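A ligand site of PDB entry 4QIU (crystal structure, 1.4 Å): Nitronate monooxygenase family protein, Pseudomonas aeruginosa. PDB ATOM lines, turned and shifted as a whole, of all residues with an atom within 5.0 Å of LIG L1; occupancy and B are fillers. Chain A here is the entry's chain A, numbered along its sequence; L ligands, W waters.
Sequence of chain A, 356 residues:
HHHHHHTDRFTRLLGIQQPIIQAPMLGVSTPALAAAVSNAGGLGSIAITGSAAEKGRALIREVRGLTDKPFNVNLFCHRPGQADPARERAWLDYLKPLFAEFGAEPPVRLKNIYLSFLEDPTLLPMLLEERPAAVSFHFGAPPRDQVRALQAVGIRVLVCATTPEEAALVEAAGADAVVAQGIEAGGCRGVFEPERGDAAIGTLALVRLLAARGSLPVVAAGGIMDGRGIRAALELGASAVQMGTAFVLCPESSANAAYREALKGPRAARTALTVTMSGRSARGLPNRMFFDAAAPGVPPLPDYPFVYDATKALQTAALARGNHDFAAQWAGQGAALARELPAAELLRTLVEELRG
The backbone NH of Leu 26 sits at hydrogen-bond distance from an oxygen (O2) of LIG L1 (2.9 Å).
The backbone NH (N) of Thr 245 is in hydrogen-bond range of an oxygen (O9) of LIG L1, 3.0 Å away.
O6 of LIG L1 lies within hydrogen-bond range of N of Gly 186, 3.4 Å away.
O2 of LG2 L2 lies within hydrogen-bond range of NE1 of Trp 330 (3.2 Å).
The backbone NH of Gly 244 sits at hydrogen-bond distance from an oxygen (O7) of LIG L1.
O9 of LIG L1 is in hydrogen-bond range of OG1 of Thr 245 (2.5 Å).
The backbone NH (N) of Gly 223 is in hydrogen-bond range of an oxygen (O8) of LIG L1 (2.8 Å).
NE2 of Gln 181 lies within hydrogen-bond range of O4 of LIG L1, at 3.0 Å.
The side-chain amide nitrogen (NE2) of Gln 242 lies within hydrogen-bond range of an oxygen (O3) of LIG L1, at 2.8 Å.
ND1 of His 138 lies close to O1 of LIG L1 (3.1 Å).
The side-chain amide oxygen (OD1) of Asn 74 sits at hydrogen-bond distance from a nitrogen (N2) of LIG L1, 3.0 Å away.
The backbone carbonyl oxygen (O) of Pro 24 lies close to a nitrogen (N3) of LIG L1 (3.2 Å).
CB of Ala 23 touches C14 of LIG L1 (3.5 Å).
Met 25 touches LIG L1.
Ala 47 touches LIG L1.
CE1 of Phe 76 touches N2 of LIG L1, at 3.5 Å.
Ala 185 touches LIG L1.
N of Gly 187 touches C9 of LIG L1 (3.8 Å).
Ala 221 touches LIG L1.
Gly 222 touches LIG L1.
CA of Met 243 touches O7 of LIG L1 (3.6 Å).
Tyr 259 touches LIG L1.
Trp 330 touches LIG L1.
CA of Gly 332 touches O8 of LIG L1, at 3.7 Å.
Hydrophobic or aromatic side chains within 4 Å of LIG L1: Ala 23, Met 25, Leu 26, Ala 47, Phe 76, His 138, Ala 185, Ala 221 and Trp 330.
22 residues have an atom within 4 Å of LIG L1: Ala 23, Pro 24, Met 25, Leu 26, Ala 47, Asn 74, Phe 76, His 138, Gln 181, Ala 185, Gly 186, Gly 187, Ala 221, Gly 222, Gly 223, Gln 242, Met 243, Gly 244, Thr 245, Tyr 259, Trp 330 and Gly 332.
The nearest printed residue that does not touch LIG L1 is Ala 331 (4.1 Å).
The backbone NH of Gly 332 lies within hydrogen-bond range of the side-chain hydroxyl of Thr 245 (2.8 Å).
O of Met 243 is in hydrogen-bond range of N of Ala 23 (2.9 Å).
The side-chain hydroxyl (OH) of Tyr 259 is in hydrogen-bond range of the backbone carbonyl oxygen (O) of Trp 330, 2.5 Å away.
Water W5 bridges an oxygen (O8) of LIG L1 (2.6 Å) and the side-chain sulfur (SD) of Met 225 (3.4 Å).
Water W3 bridges O1 of LIG L1 (2.6 Å) and ND1 of His 138 (2.8 Å).
Water W4 lies within hydrogen-bond range of O7 of LIG L1, O of Gln 242, N of Gly 222 and N of Ile 224.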
ATOM      1  N   ALA A  23     -25.845  -4.581   2.078  1.00  0.00           N
ATOM      2  CA  ALA A  23     -25.409  -3.487   2.949  1.00  0.00           C
ATOM      3  C   ALA A  23     -24.270  -3.876   3.864  1.00  0.00           C
ATOM      4  O   ALA A  23     -24.250  -4.983   4.420  1.00  0.00           O
ATOM      5  CB  ALA A  23     -26.589  -2.968   3.768  1.00  0.00           C
ATOM      6  N   PRO A  24     -23.312  -2.959   4.064  1.00  0.00           N
ATOM      7  CA  PRO A  24     -22.327  -3.178   5.120  1.00  0.00           C
ATOM      8  C   PRO A  24     -23.056  -3.166   6.437  1.00  0.00           C
ATOM      9  O   PRO A  24     -23.952  -2.338   6.625  1.00  0.00           O
ATOM     10  CB  PRO A  24     -21.405  -1.969   5.003  1.00  0.00           C
ATOM     11  CG  PRO A  24     -22.245  -0.898   4.357  1.00  0.00           C
ATOM     12  CD  PRO A  24     -23.222  -1.612   3.464  1.00  0.00           C
ATOM     13  N   MET A  25     -22.729  -4.093   7.321  1.00  0.00           N
ATOM     14  CA  MET A  25     -23.463  -4.250   8.557  1.00  0.00           C
ATOM     15  C   MET A  25     -22.512  -4.645   9.661  1.00  0.00           C
ATOM     16  O   MET A  25     -22.207  -5.831   9.824  1.00  0.00           O
ATOM     17  CB  MET A  25     -24.575  -5.302   8.413  1.00  0.00           C
ATOM     18  CG  MET A  25     -25.694  -4.914   7.423  1.00  0.00           C
ATOM     19  SD  MET A  25     -27.024  -6.146   7.354  1.00  0.00           S
ATOM     20  CE  MET A  25     -26.257  -7.361   6.264  1.00  0.00           C
ATOM     21  N   LEU A  26     -22.044  -3.667  10.433  1.00  0.00           N
ATOM     22  CA  LEU A  26     -21.041  -3.946  11.443  1.00  0.00           C
ATOM     23  C   LEU A  26     -21.532  -5.025  12.416  1.00  0.00           C
ATOM     24  O   LEU A  26     -22.584  -4.875  13.025  1.00  0.00           O
ATOM     25  CB  LEU A  26     -20.652  -2.666  12.182  1.00  0.00           C
ATOM     26  CG  LEU A  26     -19.405  -2.773  13.065  1.00  0.00           C
ATOM     27  CD1 LEU A  26     -18.176  -3.169  12.250  1.00  0.00           C
ATOM     28  CD2 LEU A  26     -19.158  -1.449  13.783  1.00  0.00           C
ATOM     29  N   VAL A  28     -22.392  -8.053  11.479  1.00  0.00           N
ATOM     30  CA  VAL A  28     -23.228  -8.988  10.728  1.00  0.00           C
ATOM     31  C   VAL A  28     -22.624  -9.338   9.368  1.00  0.00           C
ATOM     32  O   VAL A  28     -22.541 -10.513   9.011  1.00  0.00           O
ATOM     33  CB  VAL A  28     -24.652  -8.440  10.519  1.00  0.00           C
ATOM     34  CG1 VAL A  28     -25.462  -9.375   9.634  1.00  0.00           C
ATOM     35  CG2 VAL A  28     -25.349  -8.238  11.858  1.00  0.00           C
ATOM     36  N   ALA A  47     -17.981  -3.819   6.755  1.00  0.00           N
ATOM     37  CA  ALA A  47     -17.826  -2.622   7.580  1.00  0.00           C
ATOM     38  C   ALA A  47     -16.581  -2.787   8.440  1.00  0.00           C
ATOM     39  O   ALA A  47     -16.408  -3.826   9.084  1.00  0.00           O
ATOM     40  CB  ALA A  47     -19.078  -2.422   8.447  1.00  0.00           C
ATOM     41  N   ASN A  74     -16.925  -0.099   4.076  1.00  0.00           N
ATOM     42  CA  ASN A  74     -17.697   0.949   4.733  1.00  0.00           C
ATOM     43  C   ASN A  74     -17.039   1.463   6.016  1.00  0.00           C
ATOM     44  O   ASN A  74     -16.534   0.677   6.825  1.00  0.00           O
ATOM     45  CB  ASN A  74     -19.099   0.397   5.034  1.00  0.00           C
ATOM     46  CG  ASN A  74     -19.985   1.371   5.770  1.00  0.00           C
ATOM     47  OD1 ASN A  74     -20.117   1.296   6.997  1.00  0.00           O
ATOM     48  ND2 ASN A  74     -20.626   2.268   5.038  1.00  0.00           N
ATOM     49  N   PHE A  76     -17.648   4.506   9.252  1.00  0.00           N
ATOM     50  CA  PHE A  76     -18.432   5.536   9.904  1.00  0.00           C
ATOM     51  C   PHE A  76     -17.716   6.874   9.814  1.00  0.00           C
ATOM     52  O   PHE A  76     -16.496   6.938  10.016  1.00  0.00           O
ATOM     53  CB  PHE A  76     -18.695   5.207  11.378  1.00  0.00           C
ATOM     54  CG  PHE A  76     -19.504   3.947  11.591  1.00  0.00           C
ATOM     55  CD1 PHE A  76     -20.049   3.242  10.526  1.00  0.00           C
ATOM     56  CD2 PHE A  76     -19.733   3.488  12.880  1.00  0.00           C
ATOM     57  CE1 PHE A  76     -20.790   2.094  10.748  1.00  0.00           C
ATOM     58  CE2 PHE A  76     -20.474   2.341  13.102  1.00  0.00           C
ATOM     59  CZ  PHE A  76     -21.003   1.639  12.042  1.00  0.00           C
ATOM     60  N   HIS A 138     -20.949   6.481   6.296  1.00  0.00           N
ATOM     61  CA  HIS A 138     -22.210   6.584   7.019  1.00  0.00           C
ATOM     62  C   HIS A 138     -22.087   7.670   8.099  1.00  0.00           C
ATOM     63  O   HIS A 138     -21.033   7.763   8.715  1.00  0.00           O
ATOM     64  CB  HIS A 138     -22.564   5.235   7.660  1.00  0.00           C
ATOM     65  CG  HIS A 138     -24.007   5.060   7.984  1.00  0.00           C
ATOM     66  ND1 HIS A 138     -25.002   5.049   7.021  1.00  0.00           N
ATOM     67  CD2 HIS A 138     -24.639   4.878   9.178  1.00  0.00           C
ATOM     68  CE1 HIS A 138     -26.169   4.871   7.604  1.00  0.00           C
ATOM     69  NE2 HIS A 138     -25.986   4.759   8.911  1.00  0.00           N
ATOM     70  N   GLN A 181     -31.218   6.660   2.444  1.00  0.00           N
ATOM     71  CA  GLN A 181     -31.723   5.789   3.486  1.00  0.00           C
ATOM     72  C   GLN A 181     -33.053   6.292   4.037  1.00  0.00           C
ATOM     73  O   GLN A 181     -33.118   7.345   4.677  1.00  0.00           O
ATOM     74  CB  GLN A 181     -30.706   5.681   4.622  1.00  0.00           C
ATOM     75  CG  GLN A 181     -31.073   4.618   5.644  1.00  0.00           C
ATOM     76  CD  GLN A 181     -30.309   4.773   6.959  1.00  0.00           C
ATOM     77  OE1 GLN A 181     -30.255   5.865   7.533  1.00  0.00           O
ATOM     78  NE2 GLN A 181     -29.717   3.667   7.456  1.00  0.00           N
ATOM     79  N   GLU A 184     -37.596   3.382   6.810  1.00  0.00           N
ATOM     80  CA  GLU A 184     -37.753   1.918   6.863  1.00  0.00           C
ATOM     81  C   GLU A 184     -36.483   1.199   7.284  1.00  0.00           C
ATOM     82  O   GLU A 184     -36.543   0.072   7.779  1.00  0.00           O
ATOM     83  CB  GLU A 184     -38.178   1.354   5.500  1.00  0.00           C
ATOM     84  CG  GLU A 184     -39.641   1.564   5.125  1.00  0.00           C
ATOM     85  CD  GLU A 184     -39.906   2.835   4.355  1.00  0.00           C
ATOM     86  OE1 GLU A 184     -39.200   3.848   4.578  1.00  0.00           O
ATOM     87  OE2 GLU A 184     -40.841   2.817   3.534  1.00  0.00           O
ATOM     88  N   ALA A 185     -35.326   1.811   7.035  1.00  0.00           N
ATOM     89  CA  ALA A 185     -34.060   1.077   7.145  1.00  0.00           C
ATOM     90  C   ALA A 185     -33.753   0.559   8.525  1.00  0.00           C
ATOM     91  O   ALA A 185     -34.060   1.192   9.530  1.00  0.00           O
ATOM     92  CB  ALA A 185     -32.930   1.954   6.683  1.00  0.00           C
ATOM     93  N   GLY A 186     -33.141  -0.620   8.570  1.00  0.00           N
ATOM     94  CA  GLY A 186     -32.627  -1.171   9.806  1.00  0.00           C
ATOM     95  C   GLY A 186     -31.306  -0.549  10.212  1.00  0.00           C
ATOM     96  O   GLY A 186     -30.582   0.035   9.390  1.00  0.00           O
ATOM     97  N   GLY A 187     -30.957  -0.698  11.486  1.00  0.00           N
ATOM     98  CA  GLY A 187     -29.672  -0.238  11.991  1.00  0.00           C
ATOM     99  C   GLY A 187     -29.653   1.247  12.316  1.00  0.00           C
ATOM    100  O   GLY A 187     -30.711   1.895  12.416  1.00  0.00           O
ATOM    101  N   ALA A 221     -32.242   2.654  -0.127  1.00  0.00           N
ATOM    102  CA  ALA A 221     -31.979   1.790   1.029  1.00  0.00           C
ATOM    103  C   ALA A 221     -33.088   1.939   2.049  1.00  0.00           C
ATOM    104  O   ALA A 221     -33.348   3.046   2.521  1.00  0.00           O
ATOM    105  CB  ALA A 221     -30.648   2.137   1.654  1.00  0.00           C
ATOM    106  N   GLY A 222     -33.721   0.826   2.390  1.00  0.00           N
ATOM    107  CA  GLY A 222     -34.687   0.851   3.488  1.00  0.00           C
ATOM    108  C   GLY A 222     -36.005   0.185   3.123  1.00  0.00           C
ATOM    109  O   GLY A 222     -36.826   0.751   2.396  1.00  0.00           O
ATOM    110  N   GLY A 223     -36.205  -1.022   3.627  1.00  0.00           N
ATOM    111  CA  GLY A 223     -37.465  -1.710   3.462  1.00  0.00           C
ATOM    112  C   GLY A 223     -37.568  -2.608   2.237  1.00  0.00           C
ATOM    113  O   GLY A 223     -38.592  -3.257   2.026  1.00  0.00           O
ATOM    114  N   ILE A 224     -36.500  -2.659   1.449  1.00  0.00           N
ATOM    115  CA  ILE A 224     -36.505  -3.444   0.220  1.00  0.00           C
ATOM    116  C   ILE A 224     -36.080  -4.891   0.502  1.00  0.00           C
ATOM    117  O   ILE A 224     -34.980  -5.121   0.984  1.00  0.00           O
ATOM    118  CB  ILE A 224     -35.599  -2.790  -0.825  1.00  0.00           C
ATOM    119  CG1 ILE A 224     -36.148  -1.390  -1.133  1.00  0.00           C
ATOM    120  CG2 ILE A 224     -35.543  -3.640  -2.095  1.00  0.00           C
ATOM    121  CD1 ILE A 224     -35.203  -0.465  -1.885  1.00  0.00           C
ATOM    122  N   MET A 225     -36.969  -5.841   0.214  1.00  0.00           N
ATOM    123  CA  MET A 225     -36.803  -7.231   0.629  1.00  0.00           C
ATOM    124  C   MET A 225     -36.925  -8.229  -0.521  1.00  0.00           C
ATOM    125  O   MET A 225     -36.675  -9.428  -0.334  1.00  0.00           O
ATOM    126  CB  MET A 225     -37.840  -7.589   1.706  1.00  0.00           C
ATOM    127  CG  MET A 225     -37.754  -6.703   2.955  1.00  0.00           C
ATOM    128  SD  MET A 225     -36.187  -6.925   3.830  1.00  0.00           S
ATOM    129  CE  MET A 225     -36.385  -8.606   4.445  1.00  0.00           C
ATOM    130  N   GLN A 242     -29.712  -0.864  -1.931  1.00  0.00           N
ATOM    131  CA  GLN A 242     -28.855  -1.356  -0.865  1.00  0.00           C
ATOM    132  C   GLN A 242     -29.763  -2.039   0.152  1.00  0.00           C
ATOM    133  O   GLN A 242     -30.719  -1.425   0.642  1.00  0.00           O
ATOM    134  CB  GLN A 242     -28.041  -0.230  -0.228  1.00  0.00           C
ATOM    135  CG  GLN A 242     -27.139  -0.674   0.929  1.00  0.00           C
ATOM    136  CD  GLN A 242     -26.011   0.294   1.200  1.00  0.00           C
ATOM    137  OE1 GLN A 242     -25.283   0.667   0.280  1.00  0.00           O
ATOM    138  NE2 GLN A 242     -25.845   0.704   2.459  1.00  0.00           N
ATOM    139  N   MET A 243     -29.456  -3.305   0.442  1.00  0.00           N
ATOM    140  CA  MET A 243     -30.321  -4.158   1.256  1.00  0.00           C
ATOM    141  C   MET A 243     -29.545  -4.788   2.405  1.00  0.00           C
ATOM    142  O   MET A 243     -28.548  -5.488   2.175  1.00  0.00           O
ATOM    143  CB  MET A 243     -30.944  -5.264   0.373  1.00  0.00           C
ATOM    144  CG  MET A 243     -31.857  -4.706  -0.710  1.00  0.00           C
ATOM    145  SD  MET A 243     -32.273  -5.932  -1.985  1.00  0.00           S
ATOM    146  CE  MET A 243     -33.197  -7.115  -1.007  1.00  0.00           C
ATOM    147  N   GLY A 244     -29.977  -4.547   3.634  1.00  0.00           N
ATOM    148  CA  GLY A 244     -29.309  -5.095   4.803  1.00  0.00           C
ATOM    149  C   GLY A 244     -30.086  -6.246   5.413  1.00  0.00           C
ATOM    150  O   GLY A 244     -29.635  -7.394   5.428  1.00  0.00           O
ATOM    151  N   THR A 245     -31.286  -5.929   5.886  1.00  0.00           N
ATOM    152  CA  THR A 245     -32.119  -6.898   6.602  1.00  0.00           C
ATOM    153  C   THR A 245     -32.294  -8.196   5.817  1.00  0.00           C
ATOM    154  O   THR A 245     -32.234  -9.292   6.396  1.00  0.00           O
ATOM    155  CB  THR A 245     -33.484  -6.286   6.910  1.00  0.00           C
ATOM    156  OG1 THR A 245     -33.271  -5.147   7.758  1.00  0.00           O
ATOM    157  CG2 THR A 245     -34.392  -7.289   7.633  1.00  0.00           C
ATOM    158  N   ALA A 246     -32.452  -8.070   4.516  1.00  0.00           N
ATOM    159  CA  ALA A 246     -32.652  -9.243   3.657  1.00  0.00           C
ATOM    160  C   ALA A 246     -31.493 -10.252   3.718  1.00  0.00           C
ATOM    161  O   ALA A 246     -31.711 -11.431   3.454  1.00  0.00           O
ATOM    162  CB  ALA A 246     -32.895  -8.832   2.207  1.00  0.00           C
ATOM    163  N   VAL A 248     -29.384 -10.663   6.474  1.00  0.00           N
ATOM    164  CA  VAL A 248     -29.007 -11.009   7.852  1.00  0.00           C
ATOM    165  C   VAL A 248     -29.114 -12.520   8.106  1.00  0.00           C
ATOM    166  O   VAL A 248     -28.246 -13.095   8.774  1.00  0.00           O
ATOM    167  CB  VAL A 248     -29.885 -10.239   8.865  1.00  0.00           C
ATOM    168  CG1 VAL A 248     -29.664 -10.779  10.276  1.00  0.00           C
ATOM    169  CG2 VAL A 248     -29.553  -8.730   8.802  1.00  0.00           C
ATOM    170  N   TYR A 259     -30.236 -13.999  17.273  1.00  0.00           N
ATOM    171  CA  TYR A 259     -30.606 -12.980  16.281  1.00  0.00           C
ATOM    172  C   TYR A 259     -31.399 -13.617  15.135  1.00  0.00           C
ATOM    173  O   TYR A 259     -32.467 -13.124  14.732  1.00  0.00           O
ATOM    174  CB  TYR A 259     -29.335 -12.301  15.786  1.00  0.00           C
ATOM    175  CG  TYR A 259     -29.450 -11.013  14.966  1.00  0.00           C
ATOM    176  CD1 TYR A 259     -30.671 -10.486  14.561  1.00  0.00           C
ATOM    177  CD2 TYR A 259     -28.289 -10.348  14.590  1.00  0.00           C
ATOM    178  CE1 TYR A 259     -30.711  -9.303  13.803  1.00  0.00           C
ATOM    179  CE2 TYR A 259     -28.330  -9.195  13.838  1.00  0.00           C
ATOM    180  CZ  TYR A 259     -29.537  -8.671  13.450  1.00  0.00           C
ATOM    181  OH  TYR A 259     -29.531  -7.506  12.697  1.00  0.00           O
ATOM    182  N   TRP A 330     -30.746  -5.571  14.887  1.00  0.00           N
ATOM    183  CA  TRP A 330     -31.195  -4.573  13.937  1.00  0.00           C
ATOM    184  C   TRP A 330     -31.994  -5.182  12.792  1.00  0.00           C
ATOM    185  O   TRP A 330     -31.702  -6.281  12.313  1.00  0.00           O
ATOM    186  CB  TRP A 330     -30.017  -3.778  13.376  1.00  0.00           C
ATOM    187  CG  TRP A 330     -29.140  -3.061  14.358  1.00  0.00           C
ATOM    188  CD1 TRP A 330     -27.781  -2.974  14.313  1.00  0.00           C
ATOM    189  CD2 TRP A 330     -29.551  -2.258  15.469  1.00  0.00           C
ATOM    190  NE1 TRP A 330     -27.311  -2.193  15.340  1.00  0.00           N
ATOM    191  CE2 TRP A 330     -28.385  -1.734  16.058  1.00  0.00           C
ATOM    192  CE3 TRP A 330     -30.790  -1.929  16.030  1.00  0.00           C
ATOM    193  CZ2 TRP A 330     -28.410  -0.920  17.188  1.00  0.00           C
ATOM    194  CZ3 TRP A 330     -30.813  -1.107  17.149  1.00  0.00           C
ATOM    195  CH2 TRP A 330     -29.635  -0.617  17.708  1.00  0.00           C
ATOM    196  N   ALA A 331     -33.004  -4.447  12.329  1.00  0.00           N
ATOM    197  CA  ALA A 331     -33.899  -4.936  11.301  1.00  0.00           C
ATOM    198  C   ALA A 331     -34.733  -3.776  10.776  1.00  0.00           C
ATOM    199  O   ALA A 331     -35.134  -2.911  11.552  1.00  0.00           O
ATOM    200  CB  ALA A 331     -34.816  -6.057  11.840  1.00  0.00           C
ATOM    201  N   GLY A 332     -34.983  -3.798   9.471  1.00  0.00           N
ATOM    202  CA  GLY A 332     -35.791  -2.769   8.836  1.00  0.00           C
ATOM    203  C   GLY A 332     -37.272  -3.106   8.872  1.00  0.00           C
ATOM    204  O   GLY A 332     -37.671  -4.182   9.329  1.00  0.00           O
ATOM    205  N   GLN A 333     -38.096  -2.199   8.342  1.00  0.00           N
ATOM    206  CA  GLN A 333     -39.538  -2.351   8.458  1.00  0.00           C
ATOM    207  C   GLN A 333     -40.093  -3.417   7.509  1.00  0.00           C
ATOM    208  O   GLN A 333     -41.266  -3.763   7.607  1.00  0.00           O
ATOM    209  CB  GLN A 333     -40.224  -1.000   8.240  1.00  0.00           C
ATOM    210  CG  GLN A 333     -40.010  -0.045   9.428  1.00  0.00           C
ATOM    211  CD  GLN A 333     -40.731   1.282   9.241  1.00  0.00           C
ATOM    212  OE1 GLN A 333     -40.951   1.719   8.113  1.00  0.00           O
ATOM    213  NE2 GLN A 333     -41.136   1.896  10.347  1.00  0.00           N
HETATM  214  N1  LIG L   1     -25.030   0.944   7.371  1.00  0.00           N
HETATM  215  C1  LIG L   1     -23.723   1.390   7.414  1.00  0.00           C
HETATM  216  O1  LIG L   1     -23.406   2.372   6.734  1.00  0.00           O
HETATM  217  N2  LIG L   1     -22.768   0.770   8.195  1.00  0.00           N
HETATM  218  C2  LIG L   1     -23.127  -0.318   8.968  1.00  0.00           C
HETATM  219  O2  LIG L   1     -22.301  -0.889   9.683  1.00  0.00           O
HETATM  220  C3  LIG L   1     -24.446  -0.752   8.932  1.00  0.00           C
HETATM  221  N3  LIG L   1     -24.805  -1.840   9.688  1.00  0.00           N
HETATM  222  C4  LIG L   1     -26.086  -2.322   9.651  1.00  0.00           C
HETATM  223  C5  LIG L   1     -26.398  -3.428  10.429  1.00  0.00           C
HETATM  224  C6  LIG L   1     -27.682  -3.947  10.409  1.00  0.00           C
HETATM  225  C7  LIG L   1     -27.973  -5.164  11.227  1.00  0.00           C
HETATM  226  C8  LIG L   1     -28.649  -3.346   9.605  1.00  0.00           C
HETATM  227  C9  LIG L   1     -30.051  -3.896   9.588  1.00  0.00           C
HETATM  228  C10 LIG L   1     -28.335  -2.233   8.833  1.00  0.00           C
HETATM  229  C11 LIG L   1     -27.051  -1.713   8.853  1.00  0.00           C
HETATM  230  N4  LIG L   1     -26.694  -0.603   8.085  1.00  0.00           N
HETATM  231  C12 LIG L   1     -25.401  -0.132   8.133  1.00  0.00           C
HETATM  232  C13 LIG L   1     -27.724   0.092   7.248  1.00  0.00           C
HETATM  233  C14 LIG L   1     -27.721  -0.303   5.793  1.00  0.00           C
HETATM  234  O3  LIG L   1     -26.625   0.310   5.165  1.00  0.00           O
HETATM  235  C15 LIG L   1     -29.034   0.129   5.137  1.00  0.00           C
HETATM  236  O4  LIG L   1     -29.276   1.504   5.353  1.00  0.00           O
HETATM  237  C16 LIG L   1     -30.228  -0.648   5.699  1.00  0.00           C
HETATM  238  O5  LIG L   1     -29.898  -2.009   5.902  1.00  0.00           O
HETATM  239  C17 LIG L   1     -31.337  -0.585   4.646  1.00  0.00           C
HETATM  240  O6  LIG L   1     -32.544  -1.015   5.242  1.00  0.00           O
HETATM  241  P1  LIG L   1     -33.038  -2.543   5.205  1.00  0.00           P
HETATM  242  O7  LIG L   1     -32.527  -3.130   3.912  1.00  0.00           O
HETATM  243  O8  LIG L   1     -34.537  -2.506   5.328  1.00  0.00           O
HETATM  244  O9  LIG L   1     -32.376  -3.218   6.374  1.00  0.00           O
HETATM  245  C1  LG2 L   2     -24.464  -2.511  13.088  1.00  0.00           C
HETATM  246  C2  LG2 L   2     -24.413  -1.036  12.766  1.00  0.00           C
HETATM  247  C3  LG2 L   2     -24.806  -0.178  13.952  1.00  0.00           C
HETATM  248  N1  LG2 L   2     -23.978  -0.488  15.059  1.00  0.00           N
HETATM  249  O1  LG2 L   2     -22.764  -0.365  14.971  1.00  0.00           O
HETATM  250  O2  LG2 L   2     -24.466  -1.004  16.059  1.00  0.00           O
HETATM  251  O   HOH W   1     -25.893   1.240  11.174  1.00  0.00           O
HETATM  252  O   HOH W   2     -27.493   3.244   4.359  1.00  0.00           O
HETATM  253  O   HOH W   3     -24.819   3.448   4.773  1.00  0.00           O
HETATM  254  O   HOH W   4     -33.324  -1.902   1.682  1.00  0.00           O
HETATM  255  O   HOH W   5     -36.476  -4.211   5.881  1.00  0.00           O
HETATM  256  O   HOH W   6     -33.070  -5.661   3.018  1.00  0.00           O
